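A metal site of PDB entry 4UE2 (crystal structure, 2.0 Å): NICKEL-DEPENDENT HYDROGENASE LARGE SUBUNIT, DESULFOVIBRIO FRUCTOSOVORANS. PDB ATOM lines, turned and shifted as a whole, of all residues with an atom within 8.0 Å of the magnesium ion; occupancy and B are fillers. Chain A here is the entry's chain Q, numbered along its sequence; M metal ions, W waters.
OE2 of Glu 53 lies close to OE1 of Gln 494. The side-chain hydroxyl (OG1) of Thr 355 lies within hydrogen-bond range of the side-chain carboxylate (OE1) of Glu 53, at 2.7 Å. The backbone carbonyl oxygen (O) of Gly 547 lies close to a ring nitrogen (ND1) of His 549 (3.5 Å). O of Cys 546 is in hydrogen-bond range of ND1 of His 549, at 2.8 Å.
The nearest printed residue that does not touch the magnesium ion is Gln 494 (4.03 Å).
The magnesium ion is bound by water W1, water W2, water W3, the backbone carbonyl oxygen (O) of Leu 495, the side-chain carboxylate (OE2) of Glu 53 and a ring nitrogen (NE2) of His 549.
Water W3 lies within hydrogen-bond range of the side-chain carboxylate (OE1) of Glu 334 (2.5 Å), the side-chain amide oxygen (OE1) of Gln 494 (2.7 Å) and the side-chain amino group (NZ) of Lys 372 (3.1 Å). Water W2 bridges the side-chain carboxylate (OE1) of Glu 53 and the side-chain amino group (NZ) of Lys 372.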
ATOM      1  N   PHE A  49      21.069 -20.238  18.331  1.00  0.00           N
ATOM      2  CA  PHE A  49      20.387 -19.717  19.527  1.00  0.00           C
ATOM      3  C   PHE A  49      19.462 -20.801  20.089  1.00  0.00           C
ATOM      4  O   PHE A  49      18.744 -21.463  19.322  1.00  0.00           O
ATOM      5  CB  PHE A  49      19.566 -18.497  19.156  1.00  0.00           C
ATOM      6  CG  PHE A  49      18.818 -17.876  20.322  1.00  0.00           C
ATOM      7  CD1 PHE A  49      19.466 -17.016  21.193  1.00  0.00           C
ATOM      8  CD2 PHE A  49      17.476 -18.125  20.514  1.00  0.00           C
ATOM      9  CE1 PHE A  49      18.768 -16.434  22.259  1.00  0.00           C
ATOM     10  CE2 PHE A  49      16.781 -17.550  21.569  1.00  0.00           C
ATOM     11  CZ  PHE A  49      17.430 -16.712  22.447  1.00  0.00           C
ATOM     12  N   GLU A  53      17.460 -18.578  28.907  1.00  0.00           N
ATOM     13  CA  GLU A  53      16.943 -17.490  29.766  1.00  0.00           C
ATOM     14  C   GLU A  53      15.425 -17.276  29.586  1.00  0.00           C
ATOM     15  O   GLU A  53      14.715 -17.059  30.551  1.00  0.00           O
ATOM     16  CB  GLU A  53      17.712 -16.182  29.524  1.00  0.00           C
ATOM     17  CG  GLU A  53      19.239 -16.363  29.692  1.00  0.00           C
ATOM     18  CD  GLU A  53      20.067 -15.301  28.989  1.00  0.00           C
ATOM     19  OE1 GLU A  53      19.712 -14.851  27.864  1.00  0.00           O
ATOM     20  OE2 GLU A  53      21.125 -14.938  29.550  1.00  0.00           O
ATOM     21  N   GLU A 334      25.660  -5.800  29.307  1.00  0.00           N
ATOM     22  CA  GLU A 334      25.743  -6.425  27.972  1.00  0.00           C
ATOM     23  C   GLU A 334      25.065  -5.583  26.928  1.00  0.00           C
ATOM     24  O   GLU A 334      23.971  -5.048  27.177  1.00  0.00           O
ATOM     25  CB  GLU A 334      25.112  -7.830  27.969  1.00  0.00           C
ATOM     26  CG  GLU A 334      25.740  -8.804  28.947  1.00  0.00           C
ATOM     27  CD  GLU A 334      25.062 -10.169  28.917  1.00  0.00           C
ATOM     28  OE1 GLU A 334      23.955 -10.304  29.484  1.00  0.00           O
ATOM     29  OE2 GLU A 334      25.611 -11.088  28.271  1.00  0.00           O
ATOM     30  N   TYR A 341      19.376  -9.415  18.360  1.00  0.00           N
ATOM     31  CA  TYR A 341      18.363  -9.102  19.373  1.00  0.00           C
ATOM     32  C   TYR A 341      17.709  -7.788  19.016  1.00  0.00           C
ATOM     33  O   TYR A 341      18.285  -6.996  18.263  1.00  0.00           O
ATOM     34  CB  TYR A 341      18.993  -9.054  20.788  1.00  0.00           C
ATOM     35  CG  TYR A 341      19.569 -10.385  21.179  1.00  0.00           C
ATOM     36  CD1 TYR A 341      18.737 -11.445  21.564  1.00  0.00           C
ATOM     37  CD2 TYR A 341      20.947 -10.621  21.095  1.00  0.00           C
ATOM     38  CE1 TYR A 341      19.254 -12.688  21.844  1.00  0.00           C
ATOM     39  CE2 TYR A 341      21.472 -11.865  21.387  1.00  0.00           C
ATOM     40  CZ  TYR A 341      20.632 -12.888  21.770  1.00  0.00           C
ATOM     41  OH  TYR A 341      21.171 -14.127  22.046  1.00  0.00           O
ATOM     42  N   PRO A 350      23.060  -7.337  34.077  1.00  0.00           N
ATOM     43  CA  PRO A 350      22.396  -8.647  34.057  1.00  0.00           C
ATOM     44  C   PRO A 350      21.122  -8.780  34.901  1.00  0.00           C
ATOM     45  O   PRO A 350      20.235  -9.548  34.525  1.00  0.00           O
ATOM     46  CB  PRO A 350      23.489  -9.574  34.576  1.00  0.00           C
ATOM     47  CG  PRO A 350      24.750  -8.941  34.098  1.00  0.00           C
ATOM     48  CD  PRO A 350      24.514  -7.477  34.327  1.00  0.00           C
ATOM     49  N   GLY A 353      18.667  -7.790  32.611  1.00  0.00           N
ATOM     50  CA  GLY A 353      18.963  -8.375  31.317  1.00  0.00           C
ATOM     51  C   GLY A 353      17.693  -8.571  30.504  1.00  0.00           C
ATOM     52  O   GLY A 353      16.618  -8.796  31.064  1.00  0.00           O
ATOM     53  N   VAL A 354      17.827  -8.432  29.185  1.00  0.00           N
ATOM     54  CA  VAL A 354      16.722  -8.667  28.264  1.00  0.00           C
ATOM     55  C   VAL A 354      17.227  -9.605  27.166  1.00  0.00           C
ATOM     56  O   VAL A 354      18.313  -9.388  26.624  1.00  0.00           O
ATOM     57  CB  VAL A 354      16.241  -7.349  27.634  1.00  0.00           C
ATOM     58  CG1 VAL A 354      15.102  -7.611  26.650  1.00  0.00           C
ATOM     59  CG2 VAL A 354      15.762  -6.379  28.708  1.00  0.00           C
ATOM     60  N   THR A 355      16.423 -10.625  26.810  1.00  0.00           N
ATOM     61  CA  THR A 355      16.744 -11.548  25.705  1.00  0.00           C
ATOM     62  C   THR A 355      15.548 -11.639  24.722  1.00  0.00           C
ATOM     63  O   THR A 355      14.636 -12.447  24.908  1.00  0.00           O
ATOM     64  CB  THR A 355      17.091 -12.929  26.309  1.00  0.00           C
ATOM     65  OG1 THR A 355      18.093 -12.762  27.345  1.00  0.00           O
ATOM     66  CG2 THR A 355      17.593 -13.916  25.236  1.00  0.00           C
ATOM     67  N   TRP A 370      24.575 -14.325  17.535  1.00  0.00           N
ATOM     68  CA  TRP A 370      23.598 -14.658  18.566  1.00  0.00           C
ATOM     69  C   TRP A 370      24.109 -14.366  20.001  1.00  0.00           C
ATOM     70  O   TRP A 370      23.329 -14.347  20.978  1.00  0.00           O
ATOM     71  CB  TRP A 370      23.166 -16.108  18.416  1.00  0.00           C
ATOM     72  CG  TRP A 370      22.182 -16.314  17.325  1.00  0.00           C
ATOM     73  CD1 TRP A 370      22.389 -16.983  16.153  1.00  0.00           C
ATOM     74  CD2 TRP A 370      20.834 -15.837  17.290  1.00  0.00           C
ATOM     75  NE1 TRP A 370      21.254 -16.973  15.388  1.00  0.00           N
ATOM     76  CE2 TRP A 370      20.277 -16.279  16.056  1.00  0.00           C
ATOM     77  CE3 TRP A 370      20.029 -15.105  18.177  1.00  0.00           C
ATOM     78  CZ2 TRP A 370      18.961 -15.989  15.689  1.00  0.00           C
ATOM     79  CZ3 TRP A 370      18.708 -14.822  17.804  1.00  0.00           C
ATOM     80  CH2 TRP A 370      18.197 -15.263  16.567  1.00  0.00           C
ATOM     81  N   MET A 371      25.404 -14.127  20.125  1.00  0.00           N
ATOM     82  CA  MET A 371      25.955 -13.710  21.428  1.00  0.00           C
ATOM     83  C   MET A 371      25.742 -12.227  21.669  1.00  0.00           C
ATOM     84  O   MET A 371      25.794 -11.407  20.734  1.00  0.00           O
ATOM     85  CB  MET A 371      27.476 -13.964  21.530  1.00  0.00           C
ATOM     86  CG  MET A 371      27.865 -15.440  21.648  1.00  0.00           C
ATOM     87  SD  MET A 371      29.587 -15.552  22.173  1.00  0.00           S
ATOM     88  CE  MET A 371      29.967 -17.231  21.622  1.00  0.00           C
ATOM     89  N   LYS A 372      25.514 -11.873  22.935  1.00  0.00           N
ATOM     90  CA  LYS A 372      25.487 -10.492  23.338  1.00  0.00           C
ATOM     91  C   LYS A 372      26.936 -10.058  23.488  1.00  0.00           C
ATOM     92  O   LYS A 372      27.836 -10.884  23.412  1.00  0.00           O
ATOM     93  CB  LYS A 372      24.731 -10.328  24.650  1.00  0.00           C
ATOM     94  CG  LYS A 372      23.275 -10.751  24.597  1.00  0.00           C
ATOM     95  CD  LYS A 372      22.608 -10.525  25.940  1.00  0.00           C
ATOM     96  CE  LYS A 372      21.121 -10.858  25.894  1.00  0.00           C
ATOM     97  NZ  LYS A 372      20.555 -10.942  27.276  1.00  0.00           N
ATOM     98  N   PRO A 374      29.232  -8.474  26.205  1.00  0.00           N
ATOM     99  CA  PRO A 374      29.464  -8.050  27.589  1.00  0.00           C
ATOM    100  C   PRO A 374      30.606  -7.069  27.640  1.00  0.00           C
ATOM    101  O   PRO A 374      31.666  -7.293  27.030  1.00  0.00           O
ATOM    102  CB  PRO A 374      29.856  -9.361  28.301  1.00  0.00           C
ATOM    103  CG  PRO A 374      29.415 -10.469  27.378  1.00  0.00           C
ATOM    104  CD  PRO A 374      29.688  -9.877  26.021  1.00  0.00           C
ATOM    105  N   SER A 480      28.940 -15.865  35.353  1.00  0.00           N
ATOM    106  CA  SER A 480      27.992 -15.326  36.341  1.00  0.00           C
ATOM    107  C   SER A 480      26.545 -15.592  35.935  1.00  0.00           C
ATOM    108  O   SER A 480      26.175 -15.414  34.758  1.00  0.00           O
ATOM    109  CB  SER A 480      28.259 -13.837  36.617  1.00  0.00           C
ATOM    110  OG  SER A 480      28.276 -13.050  35.433  1.00  0.00           O
ATOM    111  N   TRP A 482      22.541 -14.656  37.148  1.00  0.00           N
ATOM    112  CA  TRP A 482      21.863 -13.603  37.899  1.00  0.00           C
ATOM    113  C   TRP A 482      20.372 -13.876  37.908  1.00  0.00           C
ATOM    114  O   TRP A 482      19.771 -14.043  36.841  1.00  0.00           O
ATOM    115  CB  TRP A 482      22.129 -12.250  37.226  1.00  0.00           C
ATOM    116  CG  TRP A 482      23.576 -11.969  36.891  1.00  0.00           C
ATOM    117  CD1 TRP A 482      24.325 -12.548  35.903  1.00  0.00           C
ATOM    118  CD2 TRP A 482      24.434 -11.016  37.529  1.00  0.00           C
ATOM    119  NE1 TRP A 482      25.614 -12.036  35.899  1.00  0.00           N
ATOM    120  CE2 TRP A 482      25.699 -11.089  36.885  1.00  0.00           C
ATOM    121  CE3 TRP A 482      24.263 -10.120  38.595  1.00  0.00           C
ATOM    122  CZ2 TRP A 482      26.782 -10.273  37.271  1.00  0.00           C
ATOM    123  CZ3 TRP A 482      25.353  -9.341  38.983  1.00  0.00           C
ATOM    124  CH2 TRP A 482      26.590  -9.418  38.315  1.00  0.00           C
ATOM    125  N   PHE A 493      16.201 -14.486  34.716  1.00  0.00           N
ATOM    126  CA  PHE A 493      17.401 -15.273  34.944  1.00  0.00           C
ATOM    127  C   PHE A 493      18.339 -15.041  33.766  1.00  0.00           C
ATOM    128  O   PHE A 493      17.985 -15.334  32.626  1.00  0.00           O
ATOM    129  CB  PHE A 493      17.066 -16.782  35.049  1.00  0.00           C
ATOM    130  CG  PHE A 493      18.128 -17.590  35.770  1.00  0.00           C
ATOM    131  CD1 PHE A 493      19.315 -17.896  35.133  1.00  0.00           C
ATOM    132  CD2 PHE A 493      17.947 -17.981  37.093  1.00  0.00           C
ATOM    133  CE1 PHE A 493      20.328 -18.586  35.789  1.00  0.00           C
ATOM    134  CE2 PHE A 493      18.931 -18.696  37.767  1.00  0.00           C
ATOM    135  CZ  PHE A 493      20.141 -18.997  37.107  1.00  0.00           C
ATOM    136  N   GLN A 494      19.511 -14.483  34.034  1.00  0.00           N
ATOM    137  CA  GLN A 494      20.431 -14.108  32.982  1.00  0.00           C
ATOM    138  C   GLN A 494      21.756 -14.790  33.192  1.00  0.00           C
ATOM    139  O   GLN A 494      22.237 -14.849  34.311  1.00  0.00           O
ATOM    140  CB  GLN A 494      20.623 -12.592  32.970  1.00  0.00           C
ATOM    141  CG  GLN A 494      19.362 -11.834  32.544  1.00  0.00           C
ATOM    142  CD  GLN A 494      19.045 -11.966  31.075  1.00  0.00           C
ATOM    143  OE1 GLN A 494      19.960 -12.002  30.254  1.00  0.00           O
ATOM    144  NE2 GLN A 494      17.754 -12.006  30.729  1.00  0.00           N
ATOM    145  N   LEU A 495      22.317 -15.321  32.108  1.00  0.00           N
ATOM    146  CA  LEU A 495      23.652 -15.927  32.096  1.00  0.00           C
ATOM    147  C   LEU A 495      24.573 -15.007  31.327  1.00  0.00           C
ATOM    148  O   LEU A 495      24.200 -14.482  30.268  1.00  0.00           O
ATOM    149  CB  LEU A 495      23.641 -17.293  31.374  1.00  0.00           C
ATOM    150  CG  LEU A 495      22.947 -18.473  32.053  1.00  0.00           C
ATOM    151  CD1 LEU A 495      21.442 -18.352  32.079  1.00  0.00           C
ATOM    152  CD2 LEU A 495      23.336 -19.787  31.360  1.00  0.00           C
ATOM    153  N   VAL A 496      25.780 -14.813  31.878  1.00  0.00           N
ATOM    154  CA  VAL A 496      26.852 -14.035  31.225  1.00  0.00           C
ATOM    155  C   VAL A 496      28.034 -14.974  31.349  1.00  0.00           C
ATOM    156  O   VAL A 496      28.493 -15.252  32.447  1.00  0.00           O
ATOM    157  CB  VAL A 496      27.172 -12.707  31.931  1.00  0.00           C
ATOM    158  CG1 VAL A 496      28.189 -11.901  31.113  1.00  0.00           C
ATOM    159  CG2 VAL A 496      25.887 -11.901  32.121  1.00  0.00           C
ATOM    160  N   VAL A 497      28.453 -15.511  30.213  1.00  0.00           N
ATOM    161  CA  VAL A 497      29.329 -16.681  30.180  1.00  0.00           C
ATOM    162  C   VAL A 497      30.698 -16.279  29.623  1.00  0.00           C
ATOM    163  O   VAL A 497      30.790 -15.344  28.835  1.00  0.00           O
ATOM    164  CB  VAL A 497      28.648 -17.827  29.377  1.00  0.00           C
ATOM    165  CG1 VAL A 497      29.414 -19.158  29.451  1.00  0.00           C
ATOM    166  CG2 VAL A 497      27.227 -18.032  29.883  1.00  0.00           C
ATOM    167  N   THR A 500      30.963 -15.629  26.049  1.00  0.00           N
ATOM    168  CA  THR A 500      30.275 -14.396  25.693  1.00  0.00           C
ATOM    169  C   THR A 500      31.273 -13.225  25.778  1.00  0.00           C
ATOM    170  O   THR A 500      31.337 -12.397  24.877  1.00  0.00           O
ATOM    171  CB  THR A 500      29.061 -14.112  26.608  1.00  0.00           C
ATOM    172  OG1 THR A 500      28.425 -15.340  26.944  1.00  0.00           O
ATOM    173  CG2 THR A 500      28.061 -13.233  25.892  1.00  0.00           C
ATOM    174  N   CYS A 546      27.683 -22.273  25.236  1.00  0.00           N
ATOM    175  CA  CYS A 546      27.902 -21.448  26.435  1.00  0.00           C
ATOM    176  C   CYS A 546      27.692 -19.971  26.167  1.00  0.00           C
ATOM    177  O   CYS A 546      26.942 -19.289  26.891  1.00  0.00           O
ATOM    178  CB  CYS A 546      29.335 -21.624  26.992  1.00  0.00           C
ATOM    179  SG  CYS A 546      29.516 -22.828  28.317  1.00  0.00           S
ATOM    180  N   GLY A 547      28.344 -19.471  25.117  1.00  0.00           N
ATOM    181  CA  GLY A 547      28.304 -18.031  24.822  1.00  0.00           C
ATOM    182  C   GLY A 547      26.915 -17.486  24.563  1.00  0.00           C
ATOM    183  O   GLY A 547      26.560 -16.383  25.041  1.00  0.00           O
ATOM    184  N   VAL A 548      26.131 -18.245  23.809  1.00  0.00           N
ATOM    185  CA  VAL A 548      24.758 -17.821  23.417  1.00  0.00           C
ATOM    186  C   VAL A 548      23.681 -18.294  24.381  1.00  0.00           C
ATOM    187  O   VAL A 548      22.766 -17.514  24.701  1.00  0.00           O
ATOM    188  CB  VAL A 548      24.409 -18.367  22.011  1.00  0.00           C
ATOM    189  CG1 VAL A 548      22.997 -17.959  21.635  1.00  0.00           C
ATOM    190  CG2 VAL A 548      25.411 -17.860  20.979  1.00  0.00           C
ATOM    191  N   HIS A 549      23.761 -19.564  24.808  1.00  0.00           N
ATOM    192  CA  HIS A 549      22.744 -20.191  25.660  1.00  0.00           C
ATOM    193  C   HIS A 549      21.314 -19.899  25.172  1.00  0.00           C
ATOM    194  O   HIS A 549      20.398 -19.550  25.939  1.00  0.00           O
ATOM    195  CB  HIS A 549      22.972 -19.889  27.176  1.00  0.00           C
ATOM    196  CG  HIS A 549      23.285 -18.455  27.461  1.00  0.00           C
ATOM    197  ND1 HIS A 549      24.565 -17.938  27.388  1.00  0.00           N
ATOM    198  CD2 HIS A 549      22.480 -17.430  27.839  1.00  0.00           C
ATOM    199  CE1 HIS A 549      24.523 -16.645  27.695  1.00  0.00           C
ATOM    200  NE2 HIS A 549      23.279 -16.317  27.982  1.00  0.00           N
ATOM    201  OXT HIS A 549      21.068 -20.044  23.944  1.00  0.00           O
HETATM  202 MG    MG M   1      22.917 -14.216  28.631  1.00  0.00          MG
HETATM  203  O   HOH W   1      24.588 -13.479  27.723  1.00  0.00           O
HETATM  204  O   HOH W   2      21.896 -13.801  26.898  1.00  0.00           O
HETATM  205  O   HOH W   3      22.438 -12.347  29.354  1.00  0.00           O
